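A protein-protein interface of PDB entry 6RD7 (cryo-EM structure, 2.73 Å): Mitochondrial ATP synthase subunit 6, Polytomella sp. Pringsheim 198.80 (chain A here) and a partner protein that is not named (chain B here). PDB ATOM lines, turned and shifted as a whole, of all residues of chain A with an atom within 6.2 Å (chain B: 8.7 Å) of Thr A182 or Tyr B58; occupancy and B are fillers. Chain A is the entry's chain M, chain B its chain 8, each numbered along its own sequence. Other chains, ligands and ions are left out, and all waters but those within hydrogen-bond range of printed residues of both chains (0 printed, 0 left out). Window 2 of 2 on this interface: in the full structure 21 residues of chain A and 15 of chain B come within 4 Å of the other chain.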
ATOM      1  N   THR A 175     -14.030  -0.632   1.952  1.00  0.00           N
ATOM      2  CA  THR A 175     -13.362  -1.143   0.767  1.00  0.00           C
ATOM      3  C   THR A 175     -12.199  -0.242   0.347  1.00  0.00           C
ATOM      4  O   THR A 175     -11.235  -0.709  -0.274  1.00  0.00           O
ATOM      5  CB  THR A 175     -14.431  -1.295  -0.316  1.00  0.00           C
ATOM      6  OG1 THR A 175     -15.384  -2.272   0.106  1.00  0.00           O
ATOM      7  CG2 THR A 175     -13.885  -1.769  -1.577  1.00  0.00           C
ATOM      8  N   GLY A 177     -10.016   0.739   2.305  1.00  0.00           N
ATOM      9  CA  GLY A 177      -8.863   0.121   2.927  1.00  0.00           C
ATOM     10  C   GLY A 177      -8.331  -1.018   2.076  1.00  0.00           C
ATOM     11  O   GLY A 177      -9.078  -1.701   1.376  1.00  0.00           O
ATOM     12  N   LEU A 178      -7.016  -1.229   2.151  1.00  0.00           N
ATOM     13  CA  LEU A 178      -6.348  -2.161   1.246  1.00  0.00           C
ATOM     14  C   LEU A 178      -6.678  -3.609   1.579  1.00  0.00           C
ATOM     15  O   LEU A 178      -7.075  -4.380   0.694  1.00  0.00           O
ATOM     16  CB  LEU A 178      -4.840  -1.925   1.299  1.00  0.00           C
ATOM     17  CG  LEU A 178      -3.862  -3.016   0.866  1.00  0.00           C
ATOM     18  CD1 LEU A 178      -3.889  -3.243  -0.615  1.00  0.00           C
ATOM     19  CD2 LEU A 178      -2.476  -2.626   1.279  1.00  0.00           C
ATOM     20  N   GLY A 179      -6.532  -3.989   2.850  1.00  0.00           N
ATOM     21  CA  GLY A 179      -6.667  -5.386   3.225  1.00  0.00           C
ATOM     22  C   GLY A 179      -8.081  -5.911   3.085  1.00  0.00           C
ATOM     23  O   GLY A 179      -8.279  -7.082   2.788  1.00  0.00           O
ATOM     24  N   PHE A 180      -9.071  -5.028   3.201  1.00  0.00           N
ATOM     25  CA  PHE A 180     -10.474  -5.419   3.091  1.00  0.00           C
ATOM     26  C   PHE A 180     -10.822  -5.837   1.667  1.00  0.00           C
ATOM     27  O   PHE A 180     -11.277  -6.964   1.426  1.00  0.00           O
ATOM     28  CB  PHE A 180     -11.343  -4.244   3.543  1.00  0.00           C
ATOM     29  CG  PHE A 180     -12.787  -4.582   3.785  1.00  0.00           C
ATOM     30  CD1 PHE A 180     -13.235  -4.869   5.059  1.00  0.00           C
ATOM     31  CD2 PHE A 180     -13.707  -4.557   2.749  1.00  0.00           C
ATOM     32  CE1 PHE A 180     -14.565  -5.154   5.289  1.00  0.00           C
ATOM     33  CE2 PHE A 180     -15.028  -4.852   2.973  1.00  0.00           C
ATOM     34  CZ  PHE A 180     -15.459  -5.150   4.242  1.00  0.00           C
ATOM     35  N   ALA A 181     -10.611  -4.931   0.711  1.00  0.00           N
ATOM     36  CA  ALA A 181     -10.954  -5.200  -0.679  1.00  0.00           C
ATOM     37  C   ALA A 181     -10.061  -6.283  -1.265  1.00  0.00           C
ATOM     38  O   ALA A 181     -10.529  -7.175  -1.988  1.00  0.00           O
ATOM     39  CB  ALA A 181     -10.847  -3.916  -1.491  1.00  0.00           C
ATOM     40  N   THR A 182      -8.773  -6.252  -0.923  1.00  0.00           N
ATOM     41  CA  THR A 182      -7.885  -7.274  -1.452  1.00  0.00           C
ATOM     42  C   THR A 182      -8.107  -8.612  -0.762  1.00  0.00           C
ATOM     43  O   THR A 182      -7.868  -9.662  -1.360  1.00  0.00           O
ATOM     44  CB  THR A 182      -6.440  -6.817  -1.336  1.00  0.00           C
ATOM     45  OG1 THR A 182      -6.161  -6.468   0.023  1.00  0.00           O
ATOM     46  CG2 THR A 182      -6.219  -5.619  -2.214  1.00  0.00           C
ATOM     47  N   GLY A 183      -8.642  -8.605   0.460  1.00  0.00           N
ATOM     48  CA  GLY A 183      -8.994  -9.852   1.103  1.00  0.00           C
ATOM     49  C   GLY A 183     -10.225 -10.478   0.495  1.00  0.00           C
ATOM     50  O   GLY A 183     -10.300 -11.699   0.352  1.00  0.00           O
ATOM     51  N   LEU A 184     -11.196  -9.647   0.106  1.00  0.00           N
ATOM     52  CA  LEU A 184     -12.342 -10.143  -0.654  1.00  0.00           C
ATOM     53  C   LEU A 184     -11.908 -10.736  -1.990  1.00  0.00           C
ATOM     54  O   LEU A 184     -12.372 -11.816  -2.376  1.00  0.00           O
ATOM     55  CB  LEU A 184     -13.352  -9.021  -0.874  1.00  0.00           C
ATOM     56  CG  LEU A 184     -14.073  -8.498   0.366  1.00  0.00           C
ATOM     57  CD1 LEU A 184     -14.786  -7.207   0.054  1.00  0.00           C
ATOM     58  CD2 LEU A 184     -15.044  -9.525   0.904  1.00  0.00           C
ATOM     59  N   GLY A 185     -10.981 -10.072  -2.685  1.00  0.00           N
ATOM     60  CA  GLY A 185     -10.518 -10.589  -3.968  1.00  0.00           C
ATOM     61  C   GLY A 185      -9.711 -11.872  -3.858  1.00  0.00           C
ATOM     62  O   GLY A 185      -9.920 -12.818  -4.630  1.00  0.00           O
ATOM     63  N   VAL A 186      -8.787 -11.931  -2.893  1.00  0.00           N
ATOM     64  CA  VAL A 186      -7.992 -13.136  -2.680  1.00  0.00           C
ATOM     65  C   VAL A 186      -8.876 -14.271  -2.175  1.00  0.00           C
ATOM     66  O   VAL A 186      -8.666 -15.436  -2.526  1.00  0.00           O
ATOM     67  CB  VAL A 186      -6.812 -12.822  -1.734  1.00  0.00           C
ATOM     68  CG1 VAL A 186      -6.092 -14.070  -1.260  1.00  0.00           C
ATOM     69  CG2 VAL A 186      -5.810 -11.938  -2.436  1.00  0.00           C
ATOM     70  N   SER A 187      -9.937 -13.945  -1.433  1.00  0.00           N
ATOM     71  CA  SER A 187     -10.866 -14.972  -0.978  1.00  0.00           C
ATOM     72  C   SER A 187     -11.695 -15.537  -2.121  1.00  0.00           C
ATOM     73  O   SER A 187     -11.978 -16.738  -2.142  1.00  0.00           O
ATOM     74  CB  SER A 187     -11.774 -14.402   0.099  1.00  0.00           C
ATOM     75  OG  SER A 187     -11.028 -14.064   1.248  1.00  0.00           O
ATOM     76  N   ALA A 233      -5.878 -13.320  -8.198  1.00  0.00           N
ATOM     77  CA  ALA A 233      -5.916 -13.077  -6.758  1.00  0.00           C
ATOM     78  C   ALA A 233      -5.569 -11.642  -6.418  1.00  0.00           C
ATOM     79  O   ALA A 233      -6.252 -10.999  -5.613  1.00  0.00           O
ATOM     80  CB  ALA A 233      -4.949 -14.014  -6.042  1.00  0.00           C
ATOM     81  N   VAL A 234      -4.496 -11.131  -7.012  1.00  0.00           N
ATOM     82  CA  VAL A 234      -4.151  -9.730  -6.831  1.00  0.00           C
ATOM     83  C   VAL A 234      -5.202  -8.846  -7.474  1.00  0.00           C
ATOM     84  O   VAL A 234      -5.818  -8.019  -6.797  1.00  0.00           O
ATOM     85  CB  VAL A 234      -2.747  -9.457  -7.399  1.00  0.00           C
ATOM     86  CG1 VAL A 234      -2.486  -7.969  -7.493  1.00  0.00           C
ATOM     87  CG2 VAL A 234      -1.701 -10.127  -6.530  1.00  0.00           C
ATOM     88  N   LEU A 236      -8.337  -8.962  -8.723  1.00  0.00           N
ATOM     89  CA  LEU A 236      -9.747  -8.808  -8.392  1.00  0.00           C
ATOM     90  C   LEU A 236      -9.937  -7.938  -7.156  1.00  0.00           C
ATOM     91  O   LEU A 236     -10.890  -7.159  -7.078  1.00  0.00           O
ATOM     92  CB  LEU A 236     -10.371 -10.187  -8.196  1.00  0.00           C
ATOM     93  CG  LEU A 236     -11.867 -10.230  -7.956  1.00  0.00           C
ATOM     94  CD1 LEU A 236     -12.599  -9.506  -9.054  1.00  0.00           C
ATOM     95  CD2 LEU A 236     -12.297 -11.659  -7.905  1.00  0.00           C
ATOM     96  N   GLY A 237      -9.023  -8.032  -6.193  1.00  0.00           N
ATOM     97  CA  GLY A 237      -9.130  -7.191  -5.012  1.00  0.00           C
ATOM     98  C   GLY A 237      -8.513  -5.815  -5.197  1.00  0.00           C
ATOM     99  O   GLY A 237      -9.042  -4.817  -4.702  1.00  0.00           O
ATOM    100  N   VAL A 238      -7.379  -5.743  -5.903  1.00  0.00           N
ATOM    101  CA  VAL A 238      -6.689  -4.467  -6.080  1.00  0.00           C
ATOM    102  C   VAL A 238      -7.455  -3.558  -7.046  1.00  0.00           C
ATOM    103  O   VAL A 238      -7.478  -2.335  -6.866  1.00  0.00           O
ATOM    104  CB  VAL A 238      -5.227  -4.718  -6.520  1.00  0.00           C
ATOM    105  CG1 VAL A 238      -4.476  -3.434  -6.817  1.00  0.00           C
ATOM    106  CG2 VAL A 238      -4.471  -5.440  -5.436  1.00  0.00           C
ATOM    107  N   LEU A 240     -10.565  -3.302  -7.117  1.00  0.00           N
ATOM    108  CA  LEU A 240     -11.623  -2.728  -6.307  1.00  0.00           C
ATOM    109  C   LEU A 240     -11.063  -1.706  -5.326  1.00  0.00           C
ATOM    110  O   LEU A 240     -11.662  -0.643  -5.116  1.00  0.00           O
ATOM    111  CB  LEU A 240     -12.356  -3.856  -5.585  1.00  0.00           C
ATOM    112  CG  LEU A 240     -13.541  -3.538  -4.697  1.00  0.00           C
ATOM    113  CD1 LEU A 240     -14.705  -3.031  -5.507  1.00  0.00           C
ATOM    114  CD2 LEU A 240     -13.938  -4.747  -3.864  1.00  0.00           C
ATOM    115  N   TRP A 241      -9.893  -1.999  -4.748  1.00  0.00           N
ATOM    116  CA  TRP A 241      -9.327  -1.118  -3.731  1.00  0.00           C
ATOM    117  C   TRP A 241      -8.850   0.205  -4.316  1.00  0.00           C
ATOM    118  O   TRP A 241      -9.131   1.267  -3.748  1.00  0.00           O
ATOM    119  CB  TRP A 241      -8.180  -1.807  -2.997  1.00  0.00           C
ATOM    120  CG  TRP A 241      -7.317  -0.845  -2.254  1.00  0.00           C
ATOM    121  CD1 TRP A 241      -7.700  -0.002  -1.259  1.00  0.00           C
ATOM    122  CD2 TRP A 241      -5.923  -0.616  -2.458  1.00  0.00           C
ATOM    123  NE1 TRP A 241      -6.633   0.740  -0.830  1.00  0.00           N
ATOM    124  CE2 TRP A 241      -5.526   0.379  -1.550  1.00  0.00           C
ATOM    125  CE3 TRP A 241      -4.968  -1.166  -3.312  1.00  0.00           C
ATOM    126  CZ2 TRP A 241      -4.219   0.842  -1.479  1.00  0.00           C
ATOM    127  CZ3 TRP A 241      -3.677  -0.703  -3.246  1.00  0.00           C
ATOM    128  CH2 TRP A 241      -3.311   0.289  -2.334  1.00  0.00           C
ATOM    129  N   GLY B  50     -11.724 -20.378   1.444  1.00  0.00           N
ATOM    130  CA  GLY B  50     -11.113 -19.211   0.823  1.00  0.00           C
ATOM    131  C   GLY B  50     -10.854 -18.087   1.808  1.00  0.00           C
ATOM    132  O   GLY B  50      -9.792 -17.453   1.780  1.00  0.00           O
ATOM    133  N   PHE B  51     -11.817 -17.835   2.699  1.00  0.00           N
ATOM    134  CA  PHE B  51     -11.616 -16.870   3.777  1.00  0.00           C
ATOM    135  C   PHE B  51     -10.510 -17.325   4.722  1.00  0.00           C
ATOM    136  O   PHE B  51      -9.707 -16.506   5.187  1.00  0.00           O
ATOM    137  CB  PHE B  51     -12.918 -16.666   4.548  1.00  0.00           C
ATOM    138  CG  PHE B  51     -13.959 -15.905   3.789  1.00  0.00           C
ATOM    139  CD1 PHE B  51     -13.623 -14.763   3.093  1.00  0.00           C
ATOM    140  CD2 PHE B  51     -15.277 -16.324   3.781  1.00  0.00           C
ATOM    141  CE1 PHE B  51     -14.572 -14.060   2.390  1.00  0.00           C
ATOM    142  CE2 PHE B  51     -16.233 -15.622   3.081  1.00  0.00           C
ATOM    143  CZ  PHE B  51     -15.876 -14.491   2.385  1.00  0.00           C
ATOM    144  N   THR B  52     -10.446 -18.634   4.996  1.00  0.00           N
ATOM    145  CA  THR B  52      -9.378 -19.193   5.820  1.00  0.00           C
ATOM    146  C   THR B  52      -8.013 -19.004   5.167  1.00  0.00           C
ATOM    147  O   THR B  52      -7.041 -18.630   5.839  1.00  0.00           O
ATOM    148  CB  THR B  52      -9.669 -20.674   6.070  1.00  0.00           C
ATOM    149  OG1 THR B  52     -10.838 -20.795   6.886  1.00  0.00           O
ATOM    150  CG2 THR B  52      -8.512 -21.364   6.767  1.00  0.00           C
ATOM    151  N   PHE B  53      -7.938 -19.211   3.848  1.00  0.00           N
ATOM    152  CA  PHE B  53      -6.691 -19.022   3.116  1.00  0.00           C
ATOM    153  C   PHE B  53      -6.247 -17.571   3.140  1.00  0.00           C
ATOM    154  O   PHE B  53      -5.057 -17.286   3.287  1.00  0.00           O
ATOM    155  CB  PHE B  53      -6.843 -19.494   1.670  1.00  0.00           C
ATOM    156  CG  PHE B  53      -5.636 -19.219   0.812  1.00  0.00           C
ATOM    157  CD1 PHE B  53      -4.521 -20.030   0.894  1.00  0.00           C
ATOM    158  CD2 PHE B  53      -5.618 -18.152  -0.077  1.00  0.00           C
ATOM    159  CE1 PHE B  53      -3.413 -19.782   0.111  1.00  0.00           C
ATOM    160  CE2 PHE B  53      -4.515 -17.901  -0.855  1.00  0.00           C
ATOM    161  CZ  PHE B  53      -3.414 -18.717  -0.764  1.00  0.00           C
ATOM    162  N   THR B  54      -7.188 -16.641   2.988  1.00  0.00           N
ATOM    163  CA  THR B  54      -6.810 -15.233   2.977  1.00  0.00           C
ATOM    164  C   THR B  54      -6.371 -14.761   4.355  1.00  0.00           C
ATOM    165  O   THR B  54      -5.415 -13.987   4.469  1.00  0.00           O
ATOM    166  CB  THR B  54      -7.958 -14.383   2.468  1.00  0.00           C
ATOM    167  OG1 THR B  54      -8.514 -15.008   1.312  1.00  0.00           O
ATOM    168  CG2 THR B  54      -7.457 -13.020   2.086  1.00  0.00           C
ATOM    169  N   ILE B  55      -7.030 -15.240   5.412  1.00  0.00           N
ATOM    170  CA  ILE B  55      -6.630 -14.866   6.767  1.00  0.00           C
ATOM    171  C   ILE B  55      -5.253 -15.443   7.098  1.00  0.00           C
ATOM    172  O   ILE B  55      -4.397 -14.754   7.670  1.00  0.00           O
ATOM    173  CB  ILE B  55      -7.714 -15.303   7.769  1.00  0.00           C
ATOM    174  CG1 ILE B  55      -8.949 -14.420   7.605  1.00  0.00           C
ATOM    175  CG2 ILE B  55      -7.228 -15.210   9.196  1.00  0.00           C
ATOM    176  CD1 ILE B  55     -10.208 -15.015   8.177  1.00  0.00           C
ATOM    177  N   THR B  56      -4.987 -16.678   6.660  1.00  0.00           N
ATOM    178  CA  THR B  56      -3.677 -17.293   6.869  1.00  0.00           C
ATOM    179  C   THR B  56      -2.581 -16.566   6.089  1.00  0.00           C
ATOM    180  O   THR B  56      -1.509 -16.264   6.636  1.00  0.00           O
ATOM    181  CB  THR B  56      -3.744 -18.766   6.472  1.00  0.00           C
ATOM    182  OG1 THR B  56      -4.665 -19.445   7.332  1.00  0.00           O
ATOM    183  CG2 THR B  56      -2.388 -19.426   6.585  1.00  0.00           C
ATOM    184  N   LEU B  57      -2.850 -16.244   4.820  1.00  0.00           N
ATOM    185  CA  LEU B  57      -1.863 -15.570   3.984  1.00  0.00           C
ATOM    186  C   LEU B  57      -1.584 -14.158   4.479  1.00  0.00           C
ATOM    187  O   LEU B  57      -0.438 -13.695   4.449  1.00  0.00           O
ATOM    188  CB  LEU B  57      -2.348 -15.551   2.536  1.00  0.00           C
ATOM    189  CG  LEU B  57      -1.659 -14.621   1.543  1.00  0.00           C
ATOM    190  CD1 LEU B  57      -0.330 -15.206   1.114  1.00  0.00           C
ATOM    191  CD2 LEU B  57      -2.548 -14.370   0.344  1.00  0.00           C
ATOM    192  N   TYR B  58      -2.605 -13.473   4.989  1.00  0.00           N
ATOM    193  CA  TYR B  58      -2.393 -12.110   5.455  1.00  0.00           C
ATOM    194  C   TYR B  58      -1.717 -12.105   6.818  1.00  0.00           C
ATOM    195  O   TYR B  58      -0.996 -11.162   7.153  1.00  0.00           O
ATOM    196  CB  TYR B  58      -3.716 -11.351   5.486  1.00  0.00           C
ATOM    197  CG  TYR B  58      -4.095 -10.739   4.154  1.00  0.00           C
ATOM    198  CD1 TYR B  58      -4.029 -11.481   2.983  1.00  0.00           C
ATOM    199  CD2 TYR B  58      -4.516  -9.426   4.068  1.00  0.00           C
ATOM    200  CE1 TYR B  58      -4.365 -10.941   1.780  1.00  0.00           C
ATOM    201  CE2 TYR B  58      -4.859  -8.873   2.858  1.00  0.00           C
ATOM    202  CZ  TYR B  58      -4.779  -9.642   1.722  1.00  0.00           C
ATOM    203  OH  TYR B  58      -5.111  -9.120   0.509  1.00  0.00           O
ATOM    204  N   GLY B  59      -1.895 -13.174   7.598  1.00  0.00           N
ATOM    205  CA  GLY B  59      -1.080 -13.341   8.789  1.00  0.00           C
ATOM    206  C   GLY B  59       0.381 -13.579   8.461  1.00  0.00           C
ATOM    207  O   GLY B  59       1.272 -13.074   9.151  1.00  0.00           O
ATOM    208  N   ILE B  60       0.644 -14.333   7.389  1.00  0.00           N
ATOM    209  CA  ILE B  60       2.017 -14.531   6.916  1.00  0.00           C
ATOM    210  C   ILE B  60       2.630 -13.208   6.456  1.00  0.00           C
ATOM    211  O   ILE B  60       3.786 -12.895   6.773  1.00  0.00           O
ATOM    212  CB  ILE B  60       2.038 -15.595   5.802  1.00  0.00           C
ATOM    213  CG1 ILE B  60       1.722 -16.971   6.382  1.00  0.00           C
ATOM    214  CG2 ILE B  60       3.374 -15.638   5.093  1.00  0.00           C
ATOM    215  CD1 ILE B  60       1.538 -18.037   5.336  1.00  0.00           C
ATOM    216  N   LEU B  61       1.853 -12.397   5.734  1.00  0.00           N
ATOM    217  CA  LEU B  61       2.354 -11.108   5.262  1.00  0.00           C
ATOM    218  C   LEU B  61       2.570 -10.128   6.413  1.00  0.00           C
ATOM    219  O   LEU B  61       3.516  -9.329   6.388  1.00  0.00           O
ATOM    220  CB  LEU B  61       1.396 -10.517   4.231  1.00  0.00           C
ATOM    221  CG  LEU B  61       1.243 -11.286   2.920  1.00  0.00           C
ATOM    222  CD1 LEU B  61       0.385 -10.506   1.942  1.00  0.00           C
ATOM    223  CD2 LEU B  61       2.596 -11.597   2.316  1.00  0.00           C
ATOM    224  N   ASP B  62       1.720 -10.189   7.440  1.00  0.00           N
ATOM    225  CA  ASP B  62       1.933  -9.370   8.630  1.00  0.00           C
ATOM    226  C   ASP B  62       3.177  -9.808   9.389  1.00  0.00           C
ATOM    227  O   ASP B  62       3.898  -8.972   9.945  1.00  0.00           O
ATOM    228  CB  ASP B  62       0.710  -9.437   9.541  1.00  0.00           C
ATOM    229  CG  ASP B  62      -0.345  -8.422   9.174  1.00  0.00           C
ATOM    230  OD1 ASP B  62       0.011  -7.388   8.573  1.00  0.00           O
ATOM    231  OD2 ASP B  62      -1.527  -8.655   9.492  1.00  0.00           O
ATOM    232  N   GLY B  63       3.444 -11.116   9.419  1.00  0.00           N
ATOM    233  CA  GLY B  63       4.677 -11.597  10.022  1.00  0.00           C
ATOM    234  C   GLY B  63       5.913 -11.144   9.269  1.00  0.00           C
ATOM    235  O   GLY B  63       6.929 -10.801   9.881  1.00  0.00           O
ATOM    236  N   LEU B  64       5.835 -11.117   7.935  1.00  0.00           N
ATOM    237  CA  LEU B  64       6.944 -10.610   7.125  1.00  0.00           C
ATOM    238  C   LEU B  64       7.177  -9.124   7.370  1.00  0.00           C
ATOM    239  O   LEU B  64       8.326  -8.676   7.484  1.00  0.00           O
ATOM    240  CB  LEU B  64       6.674 -10.859   5.642  1.00  0.00           C
ATOM    241  CG  LEU B  64       6.667 -12.293   5.122  1.00  0.00           C
ATOM    242  CD1 LEU B  64       6.711 -12.288   3.609  1.00  0.00           C
ATOM    243  CD2 LEU B  64       7.828 -13.082   5.689  1.00  0.00           C
ATOM    244  N   ARG B  65       6.093  -8.351   7.466  1.00  0.00           N
ATOM    245  CA  ARG B  65       6.205  -6.919   7.727  1.00  0.00           C
ATOM    246  C   ARG B  65       6.793  -6.649   9.109  1.00  0.00           C
ATOM    247  O   ARG B  65       7.640  -5.760   9.279  1.00  0.00           O
ATOM    248  CB  ARG B  65       4.831  -6.269   7.592  1.00  0.00           C
ATOM    249  CG  ARG B  65       4.832  -4.768   7.700  1.00  0.00           C
ATOM    250  CD  ARG B  65       3.822  -4.174   6.753  1.00  0.00           C
ATOM    251  NE  ARG B  65       2.451  -4.383   7.208  1.00  0.00           N
ATOM    252  CZ  ARG B  65       1.703  -3.444   7.776  1.00  0.00           C
ATOM    253  NH1 ARG B  65       0.464  -3.722   8.156  1.00  0.00           N
ATOM    254  NH2 ARG B  65       2.192  -2.227   7.964  1.00  0.00           N
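The side-chain hydroxyl (OG1) of Thr B54 lies within hydrogen-bond range of the side-chain hydroxyl (OG) of Ser A187 (2.7 Å). OG1 of Thr A182 lies within hydrogen-bond range of OH of Tyr B58 (2.9 Å).
The side-chain hydroxyl (OG1) of Thr B54 lies within hydrogen-bond range of the backbone carbonyl oxygen (O) of Gly B50 (2.8 Å). The side-chain hydroxyl of Ser A187 lies within hydrogen-bond range of the backbone carbonyl oxygen of Gly A183, at 2.6 Å.
Tyr B58 touches Gly A179 (CE2 to O, 3.9 Å). Thr B54 touches Gly A183. N of Gly A183 touches OH of Tyr B58, at 3.6 Å. Val A186 touches Thr B54 (C to OG1, 3.6 Å). Val A186 touches Leu B57 (CG1 to CD2, 3.9 Å). Gly B50 touches Ser A187. OG of Ser A187 touches CD1 of Phe B51, 3.3 Å away.
Of chain B, only Thr B54 (3.6 Å) and Tyr B58 (3.6 Å) come within 4 Å of Gly A183. Of the printed residues of chain B, Val A186 touches Thr B54 and Leu B57. Gly A237 touches none of the printed residues of chain B. Of the printed residues of chain A, Gly B50 touches Ser A187. Printed residues of chain A within 4 Å of Thr B54: Gly A183, Val A186 and Ser A187. Of the printed residues of chain A, Leu B57 touches Val A186 (3.9 Å). The nearest residue of chain B that does not touch Thr A182 is Thr B54 (4.8 Å). The nearest residue of chain A that does not touch Tyr B58 is Val A186 (4.1 Å). The nearest printed residue of chain B that does not touch Ser A187 is Ile B55 (5.9 Å).
Printed residues of chain B that touch a printed residue of chain A: Gly B50, Phe B51, Thr B54, Leu B57 and Tyr B58. Hydrophobic or aromatic side chains of chain B within 4 Å of the printed part of chain A: Phe B51, Leu B57 and Tyr B58. Printed residues of chain A that touch a printed residue of chain B: Gly A179, Thr A182, Gly A183, Val A186 and Ser A187. Among the printed residues, no Asp or Glu carboxylate lies within 4 Å of a Lys or Arg side-chain nitrogen of the other chain.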
